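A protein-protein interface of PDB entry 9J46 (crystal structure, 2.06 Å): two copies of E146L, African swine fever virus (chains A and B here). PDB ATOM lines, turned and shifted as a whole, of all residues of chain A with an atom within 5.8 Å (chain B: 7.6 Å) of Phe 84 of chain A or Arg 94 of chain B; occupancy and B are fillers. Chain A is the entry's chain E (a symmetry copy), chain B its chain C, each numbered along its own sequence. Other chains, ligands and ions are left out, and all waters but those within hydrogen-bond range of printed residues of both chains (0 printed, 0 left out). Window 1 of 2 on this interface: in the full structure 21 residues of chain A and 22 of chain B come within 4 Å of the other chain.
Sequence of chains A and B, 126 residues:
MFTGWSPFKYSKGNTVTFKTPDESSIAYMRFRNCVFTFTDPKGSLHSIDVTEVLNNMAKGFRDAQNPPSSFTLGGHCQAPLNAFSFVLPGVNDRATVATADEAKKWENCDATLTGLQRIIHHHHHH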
ATOM      1  N   PHE A  36      29.173  19.704  36.108  1.00  0.00           N
ATOM      2  CA  PHE A  36      29.656  19.312  34.801  1.00  0.00           C
ATOM      3  C   PHE A  36      30.909  20.122  34.513  1.00  0.00           C
ATOM      4  O   PHE A  36      30.911  21.345  34.667  1.00  0.00           O
ATOM      5  CB  PHE A  36      28.584  19.530  33.730  1.00  0.00           C
ATOM      6  CG  PHE A  36      29.068  19.261  32.342  1.00  0.00           C
ATOM      7  CD1 PHE A  36      29.417  17.974  31.958  1.00  0.00           C
ATOM      8  CD2 PHE A  36      29.200  20.292  31.430  1.00  0.00           C
ATOM      9  CE1 PHE A  36      29.882  17.730  30.677  1.00  0.00           C
ATOM     10  CE2 PHE A  36      29.656  20.058  30.144  1.00  0.00           C
ATOM     11  CZ  PHE A  36      29.997  18.775  29.766  1.00  0.00           C
ATOM     12  N   ASN A  82      30.165  14.357  26.557  1.00  0.00           N
ATOM     13  CA  ASN A  82      31.121  15.160  25.804  1.00  0.00           C
ATOM     14  C   ASN A  82      31.061  16.589  26.329  1.00  0.00           C
ATOM     15  O   ASN A  82      30.278  16.906  27.229  1.00  0.00           O
ATOM     16  CB  ASN A  82      30.808  15.110  24.309  1.00  0.00           C
ATOM     17  CG  ASN A  82      29.434  15.660  24.008  1.00  0.00           C
ATOM     18  OD1 ASN A  82      29.271  16.866  23.831  1.00  0.00           O
ATOM     19  ND2 ASN A  82      28.422  14.786  24.015  1.00  0.00           N
ATOM     20  N   ALA A  83      31.881  17.464  25.755  1.00  0.00           N
ATOM     21  CA  ALA A  83      31.980  18.820  26.280  1.00  0.00           C
ATOM     22  C   ALA A  83      30.693  19.631  26.108  1.00  0.00           C
ATOM     23  O   ALA A  83      30.540  20.677  26.758  1.00  0.00           O
ATOM     24  CB  ALA A  83      33.145  19.555  25.611  1.00  0.00           C
ATOM     25  N   PHE A  84      29.766  19.192  25.255  1.00  0.00           N
ATOM     26  CA  PHE A  84      28.517  19.910  25.022  1.00  0.00           C
ATOM     27  C   PHE A  84      27.326  19.244  25.682  1.00  0.00           C
ATOM     28  O   PHE A  84      26.192  19.586  25.348  1.00  0.00           O
ATOM     29  CB  PHE A  84      28.251  20.050  23.517  1.00  0.00           C
ATOM     30  CG  PHE A  84      29.291  20.858  22.809  1.00  0.00           C
ATOM     31  CD1 PHE A  84      29.245  22.243  22.836  1.00  0.00           C
ATOM     32  CD2 PHE A  84      30.349  20.237  22.164  1.00  0.00           C
ATOM     33  CE1 PHE A  84      30.220  23.000  22.199  1.00  0.00           C
ATOM     34  CE2 PHE A  84      31.327  20.986  21.524  1.00  0.00           C
ATOM     35  CZ  PHE A  84      31.261  22.369  21.541  1.00  0.00           C
ATOM     36  N   SER A  85      27.546  18.292  26.594  1.00  0.00           N
ATOM     37  CA  SER A  85      26.418  17.614  27.221  1.00  0.00           C
ATOM     38  C   SER A  85      25.570  18.572  28.042  1.00  0.00           C
ATOM     39  O   SER A  85      24.380  18.315  28.247  1.00  0.00           O
ATOM     40  CB  SER A  85      26.901  16.473  28.108  1.00  0.00           C
ATOM     41  OG  SER A  85      27.524  15.480  27.332  1.00  0.00           O
ATOM     42  N   PHE A  86      26.166  19.656  28.542  1.00  0.00           N
ATOM     43  CA  PHE A  86      25.441  20.696  29.258  1.00  0.00           C
ATOM     44  C   PHE A  86      25.984  22.049  28.823  1.00  0.00           C
ATOM     45  O   PHE A  86      27.151  22.166  28.428  1.00  0.00           O
ATOM     46  CB  PHE A  86      25.570  20.567  30.782  1.00  0.00           C
ATOM     47  CG  PHE A  86      25.082  19.278  31.326  1.00  0.00           C
ATOM     48  CD1 PHE A  86      25.922  18.178  31.390  1.00  0.00           C
ATOM     49  CD2 PHE A  86      23.785  19.159  31.797  1.00  0.00           C
ATOM     50  CE1 PHE A  86      25.478  16.981  31.912  1.00  0.00           C
ATOM     51  CE2 PHE A  86      23.331  17.954  32.331  1.00  0.00           C
ATOM     52  CZ  PHE A  86      24.185  16.865  32.386  1.00  0.00           C
ATOM     53  N   VAL A  87      25.136  23.077  28.918  1.00  0.00           N
ATOM     54  CA  VAL A  87      25.463  24.411  28.426  1.00  0.00           C
ATOM     55  C   VAL A  87      26.002  25.265  29.563  1.00  0.00           C
ATOM     56  O   VAL A  87      25.356  25.393  30.614  1.00  0.00           O
ATOM     57  CB  VAL A  87      24.241  25.097  27.801  1.00  0.00           C
ATOM     58  CG1 VAL A  87      24.553  26.577  27.611  1.00  0.00           C
ATOM     59  CG2 VAL A  87      23.901  24.464  26.480  1.00  0.00           C
ATOM     60  N   ASN A  92      30.005  27.352  25.759  1.00  0.00           N
ATOM     61  CA  ASN A  92      29.795  26.263  24.807  1.00  0.00           C
ATOM     62  C   ASN A  92      28.372  26.256  24.256  1.00  0.00           C
ATOM     63  O   ASN A  92      27.864  25.193  23.896  1.00  0.00           O
ATOM     64  CB  ASN A  92      30.117  24.904  25.446  1.00  0.00           C
ATOM     65  CG  ASN A  92      29.183  24.578  26.588  1.00  0.00           C
ATOM     66  OD1 ASN A  92      28.436  25.447  27.050  1.00  0.00           O
ATOM     67  ND2 ASN A  92      29.209  23.339  27.049  1.00  0.00           N
ATOM     68  N   ASP A  93      27.704  27.410  24.213  1.00  0.00           N
ATOM     69  CA  ASP A  93      26.336  27.466  23.721  1.00  0.00           C
ATOM     70  C   ASP A  93      26.331  27.657  22.205  1.00  0.00           C
ATOM     71  O   ASP A  93      27.370  27.819  21.563  1.00  0.00           O
ATOM     72  CB  ASP A  93      25.529  28.584  24.400  1.00  0.00           C
ATOM     73  CG  ASP A  93      26.217  29.942  24.321  1.00  0.00           C
ATOM     74  OD1 ASP A  93      26.892  30.235  23.317  1.00  0.00           O
ATOM     75  OD2 ASP A  93      26.067  30.751  25.265  1.00  0.00           O
ATOM     76  N   VAL A  97      29.565  28.518  19.815  1.00  0.00           N
ATOM     77  CA  VAL A  97      30.002  27.454  18.918  1.00  0.00           C
ATOM     78  C   VAL A  97      28.886  27.238  17.898  1.00  0.00           C
ATOM     79  O   VAL A  97      28.028  26.361  18.076  1.00  0.00           O
ATOM     80  CB  VAL A  97      30.312  26.155  19.695  1.00  0.00           C
ATOM     81  CG1 VAL A  97      30.817  25.048  18.755  1.00  0.00           C
ATOM     82  CG2 VAL A  97      31.312  26.417  20.825  1.00  0.00           C
ATOM     83  N   ALA A 103      32.756  23.694  15.944  1.00  0.00           N
ATOM     84  CA  ALA A 103      32.534  22.557  16.828  1.00  0.00           C
ATOM     85  C   ALA A 103      33.593  21.479  16.640  1.00  0.00           C
ATOM     86  O   ALA A 103      33.900  20.737  17.584  1.00  0.00           O
ATOM     87  CB  ALA A 103      31.140  21.972  16.596  1.00  0.00           C
ATOM     88  N   TRP A 106      36.603  21.327  18.894  1.00  0.00           N
ATOM     89  CA  TRP A 106      36.295  20.913  20.254  1.00  0.00           C
ATOM     90  C   TRP A 106      36.298  19.407  20.425  1.00  0.00           C
ATOM     91  O   TRP A 106      35.990  18.930  21.520  1.00  0.00           O
ATOM     92  CB  TRP A 106      34.914  21.436  20.672  1.00  0.00           C
ATOM     93  CG  TRP A 106      34.810  22.909  20.998  1.00  0.00           C
ATOM     94  CD1 TRP A 106      34.913  23.967  20.128  1.00  0.00           C
ATOM     95  CD2 TRP A 106      34.537  23.476  22.289  1.00  0.00           C
ATOM     96  NE1 TRP A 106      34.739  25.157  20.810  1.00  0.00           N
ATOM     97  CE2 TRP A 106      34.502  24.880  22.133  1.00  0.00           C
ATOM     98  CE3 TRP A 106      34.330  22.930  23.562  1.00  0.00           C
ATOM     99  CZ2 TRP A 106      34.277  25.746  23.208  1.00  0.00           C
ATOM    100  CZ3 TRP A 106      34.094  23.793  24.633  1.00  0.00           C
ATOM    101  CH2 TRP A 106      34.072  25.189  24.445  1.00  0.00           C
ATOM    102  N   GLY B  75      26.997  21.862  14.567  1.00  0.00           N
ATOM    103  CA  GLY B  75      27.224  21.553  15.965  1.00  0.00           C
ATOM    104  C   GLY B  75      28.216  20.405  16.108  1.00  0.00           C
ATOM    105  O   GLY B  75      28.845  19.951  15.143  1.00  0.00           O
ATOM    106  N   HIS B  76      28.345  19.922  17.349  1.00  0.00           N
ATOM    107  CA  HIS B  76      29.370  18.917  17.623  1.00  0.00           C
ATOM    108  C   HIS B  76      29.031  17.571  17.000  1.00  0.00           C
ATOM    109  O   HIS B  76      29.932  16.745  16.797  1.00  0.00           O
ATOM    110  CB  HIS B  76      29.595  18.763  19.137  1.00  0.00           C
ATOM    111  CG  HIS B  76      28.639  17.824  19.812  1.00  0.00           C
ATOM    112  ND1 HIS B  76      27.303  18.123  19.997  1.00  0.00           N
ATOM    113  CD2 HIS B  76      28.833  16.605  20.371  1.00  0.00           C
ATOM    114  CE1 HIS B  76      26.712  17.121  20.622  1.00  0.00           C
ATOM    115  NE2 HIS B  76      27.617  16.187  20.861  1.00  0.00           N
ATOM    116  N   CYS B  77      27.756  17.339  16.684  1.00  0.00           N
ATOM    117  CA  CYS B  77      27.355  16.081  16.075  1.00  0.00           C
ATOM    118  C   CYS B  77      27.916  15.920  14.667  1.00  0.00           C
ATOM    119  O   CYS B  77      27.967  14.790  14.159  1.00  0.00           O
ATOM    120  CB  CYS B  77      25.829  15.990  16.046  1.00  0.00           C
ATOM    121  SG  CYS B  77      25.060  15.545  17.630  1.00  0.00           S
ATOM    122  N   PHE B  84      16.570  19.659  14.746  1.00  0.00           N
ATOM    123  CA  PHE B  84      17.219  20.420  15.812  1.00  0.00           C
ATOM    124  C   PHE B  84      18.293  21.351  15.287  1.00  0.00           C
ATOM    125  O   PHE B  84      19.087  21.871  16.079  1.00  0.00           O
ATOM    126  CB  PHE B  84      17.823  19.477  16.854  1.00  0.00           C
ATOM    127  CG  PHE B  84      16.803  18.652  17.539  1.00  0.00           C
ATOM    128  CD1 PHE B  84      16.024  19.191  18.535  1.00  0.00           C
ATOM    129  CD2 PHE B  84      16.584  17.348  17.153  1.00  0.00           C
ATOM    130  CE1 PHE B  84      15.070  18.442  19.150  1.00  0.00           C
ATOM    131  CE2 PHE B  84      15.626  16.598  17.764  1.00  0.00           C
ATOM    132  CZ  PHE B  84      14.865  17.139  18.760  1.00  0.00           C
ATOM    133  N   VAL B  87      16.900  26.395  16.818  1.00  0.00           N
ATOM    134  CA  VAL B  87      16.064  26.338  18.007  1.00  0.00           C
ATOM    135  C   VAL B  87      14.844  27.215  17.813  1.00  0.00           C
ATOM    136  O   VAL B  87      14.963  28.401  17.485  1.00  0.00           O
ATOM    137  CB  VAL B  87      16.837  26.794  19.258  1.00  0.00           C
ATOM    138  CG1 VAL B  87      15.893  26.805  20.455  1.00  0.00           C
ATOM    139  CG2 VAL B  87      18.036  25.905  19.505  1.00  0.00           C
ATOM    140  N   GLY B  90      10.698  26.698  23.310  1.00  0.00           N
ATOM    141  CA  GLY B  90       9.506  26.014  23.777  1.00  0.00           C
ATOM    142  C   GLY B  90       9.117  24.779  22.974  1.00  0.00           C
ATOM    143  O   GLY B  90       8.194  24.060  23.377  1.00  0.00           O
ATOM    144  N   VAL B  91       9.810  24.492  21.875  1.00  0.00           N
ATOM    145  CA  VAL B  91       9.402  23.420  20.969  1.00  0.00           C
ATOM    146  C   VAL B  91      10.487  22.357  20.813  1.00  0.00           C
ATOM    147  O   VAL B  91      10.256  21.178  21.119  1.00  0.00           O
ATOM    148  CB  VAL B  91       9.009  23.981  19.590  1.00  0.00           C
ATOM    149  CG1 VAL B  91       8.723  22.827  18.638  1.00  0.00           C
ATOM    150  CG2 VAL B  91       7.805  24.961  19.711  1.00  0.00           C
ATOM    151  N   ASN B  92      11.666  22.739  20.313  1.00  0.00           N
ATOM    152  CA  ASN B  92      12.741  21.768  20.146  1.00  0.00           C
ATOM    153  C   ASN B  92      14.011  22.176  20.879  1.00  0.00           C
ATOM    154  O   ASN B  92      15.110  21.907  20.393  1.00  0.00           O
ATOM    155  CB  ASN B  92      13.055  21.548  18.666  1.00  0.00           C
ATOM    156  CG  ASN B  92      13.576  22.778  18.016  1.00  0.00           C
ATOM    157  OD1 ASN B  92      13.526  23.865  18.608  1.00  0.00           O
ATOM    158  ND2 ASN B  92      14.117  22.635  16.805  1.00  0.00           N
ATOM    159  N   ASP B  93      13.894  22.834  22.028  1.00  0.00           N
ATOM    160  CA  ASP B  93      15.105  23.233  22.731  1.00  0.00           C
ATOM    161  C   ASP B  93      15.484  22.172  23.776  1.00  0.00           C
ATOM    162  O   ASP B  93      14.810  21.145  23.939  1.00  0.00           O
ATOM    163  CB  ASP B  93      14.964  24.628  23.361  1.00  0.00           C
ATOM    164  CG  ASP B  93      13.700  24.801  24.193  1.00  0.00           C
ATOM    165  OD1 ASP B  93      13.223  23.850  24.839  1.00  0.00           O
ATOM    166  OD2 ASP B  93      13.220  25.954  24.271  1.00  0.00           O
ATOM    167  N   ARG B  94      16.595  22.416  24.488  1.00  0.00           N
ATOM    168  CA  ARG B  94      17.109  21.424  25.433  1.00  0.00           C
ATOM    169  C   ARG B  94      16.161  21.208  26.596  1.00  0.00           C
ATOM    170  O   ARG B  94      16.059  20.099  27.115  1.00  0.00           O
ATOM    171  CB  ARG B  94      18.465  21.845  25.990  1.00  0.00           C
ATOM    172  CG  ARG B  94      19.606  21.746  25.039  1.00  0.00           C
ATOM    173  CD  ARG B  94      20.830  22.159  25.797  1.00  0.00           C
ATOM    174  NE  ARG B  94      22.036  22.075  24.993  1.00  0.00           N
ATOM    175  CZ  ARG B  94      23.044  21.246  25.227  1.00  0.00           C
ATOM    176  NH1 ARG B  94      22.969  20.308  26.164  1.00  0.00           N
ATOM    177  NH2 ARG B  94      24.166  21.380  24.521  1.00  0.00           N
ATOM    178  N   ALA B  95      15.507  22.262  27.066  1.00  0.00           N
ATOM    179  CA  ALA B  95      14.526  22.064  28.126  1.00  0.00           C
ATOM    180  C   ALA B  95      13.370  21.192  27.637  1.00  0.00           C
ATOM    181  O   ALA B  95      12.907  20.293  28.353  1.00  0.00           O
ATOM    182  CB  ALA B  95      14.027  23.422  28.631  1.00  0.00           C
ATOM    183  N   THR B  96      12.920  21.396  26.398  1.00  0.00           N
ATOM    184  CA  THR B  96      11.805  20.580  25.903  1.00  0.00           C
ATOM    185  C   THR B  96      12.244  19.174  25.511  1.00  0.00           C
ATOM    186  O   THR B  96      11.541  18.197  25.803  1.00  0.00           O
ATOM    187  CB  THR B  96      11.132  21.279  24.722  1.00  0.00           C
ATOM    188  OG1 THR B  96      10.950  22.646  25.061  1.00  0.00           O
ATOM    189  CG2 THR B  96       9.742  20.658  24.434  1.00  0.00           C
ATOM    190  N   VAL B  97      13.387  19.031  24.858  1.00  0.00           N
ATOM    191  CA  VAL B  97      13.885  17.720  24.439  1.00  0.00           C
ATOM    192  C   VAL B  97      15.204  17.490  25.177  1.00  0.00           C
ATOM    193  O   VAL B  97      16.283  17.800  24.668  1.00  0.00           O
ATOM    194  CB  VAL B  97      14.054  17.626  22.920  1.00  0.00           C
ATOM    195  CG1 VAL B  97      14.370  16.201  22.520  1.00  0.00           C
ATOM    196  CG2 VAL B  97      12.766  18.093  22.230  1.00  0.00           C
ATOM    197  N   ALA B  98      15.128  16.916  26.384  1.00  0.00           N
ATOM    198  CA  ALA B  98      16.245  16.974  27.320  1.00  0.00           C
ATOM    199  C   ALA B  98      17.035  15.684  27.440  1.00  0.00           C
ATOM    200  O   ALA B  98      18.184  15.729  27.892  1.00  0.00           O
ATOM    201  CB  ALA B  98      15.748  17.382  28.719  1.00  0.00           C
ATOM    202  N   THR B  99      16.468  14.549  27.045  1.00  0.00           N
ATOM    203  CA  THR B  99      17.113  13.250  27.177  1.00  0.00           C
ATOM    204  C   THR B  99      17.221  12.567  25.821  1.00  0.00           C
ATOM    205  O   THR B  99      16.486  12.881  24.879  1.00  0.00           O
ATOM    206  CB  THR B  99      16.333  12.333  28.126  1.00  0.00           C
ATOM    207  OG1 THR B  99      14.980  12.200  27.658  1.00  0.00           O
ATOM    208  CG2 THR B  99      16.330  12.898  29.524  1.00  0.00           C
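CB of His 76 of chain B touches CD2 of Phe 84 of chain A, at 3.5 Å.
Phe 86 of chain A touches Arg 94 of chain B.
Val 87 of chain A touches Arg 94 of chain B.
Gly 75 of chain B touches Ala 103 of chain A (C to CB, 3.4 Å).
CB of Ala 103 of chain A touches N of His 76 of chain B (3.5 Å).
Phe 84 of chain A touches just these residues of chain B: His 76 (3.5 Å) and Arg 94 (2.8 Å).
Of chain A, only Phe 84, Ser 85, Phe 86 and Val 87 come within 4 Å of Arg 94 of chain B.
No residue of chain B comes within 4 Å of Ala 83 of chain A.
Of the printed residues of chain B, Ser 85 of chain A touches Arg 94.
Printed residues of chain A within 4 Å of Gly 75 of chain B: Ala 103.
Of the printed residues of chain B, Asn 82 of chain A touches His 76 (3.5 Å).
The nearest residue of chain B that does not touch Phe 84 of chain A is Gly 75 of chain B (6.3 Å).
The nearest residue of chain A that does not touch Arg 94 of chain B is Asn 92 of chain A (5.3 Å).
The nearest printed residue of chain A that does not touch His 76 of chain B is Val 97 of chain A (5.9 Å).
O of Ser 85 of chain A is in hydrogen-bond range of NH1 of Arg 94 of chain B, at 3.2 Å.
The backbone carbonyl oxygen of Phe 84 of chain A is in hydrogen-bond range of the guanidinium group of Arg 94 of chain B, 2.8 Å away.
NE2 of His 76 of chain B lies within hydrogen-bond range of OD1 of Asn 82 of chain A (3.5 Å).
Hydrophobic or aromatic side chains of chain A within 4 Å of the printed part of chain B: Phe 84, Val 87 and Ala 103.
Printed residues of chain B that touch a printed residue of chain A: Gly 75, His 76 and Arg 94.
Hydrophobic or aromatic side chains of chain B within 4 Å of the printed part of chain A: His 76.
Among the printed residues, 8 pairs touch across the chains.
Among the printed residues, no Asp or Glu carboxylate lies within 4 Å of a Lys or Arg side-chain nitrogen of the other chain.
The side-chain amide oxygen (OD1) of Asn 82 of chain A is in hydrogen-bond range of the backbone NH (N) of Phe 84 of chain A (2.8 Å).
OG of Ser 85 of chain A lies within hydrogen-bond range of N of Asn 82 of chain A, at 3.0 Å.
The backbone carbonyl oxygen (O) of Phe 86 of chain A sits at hydrogen-bond distance from the side-chain amide nitrogen (ND2) of Asn 92 of chain A (2.7 Å).
5 positions are printed for both chains.
Of the 8 pairs that touch across the chains among the printed residues, none has its exchanged pair printed and touching as well.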
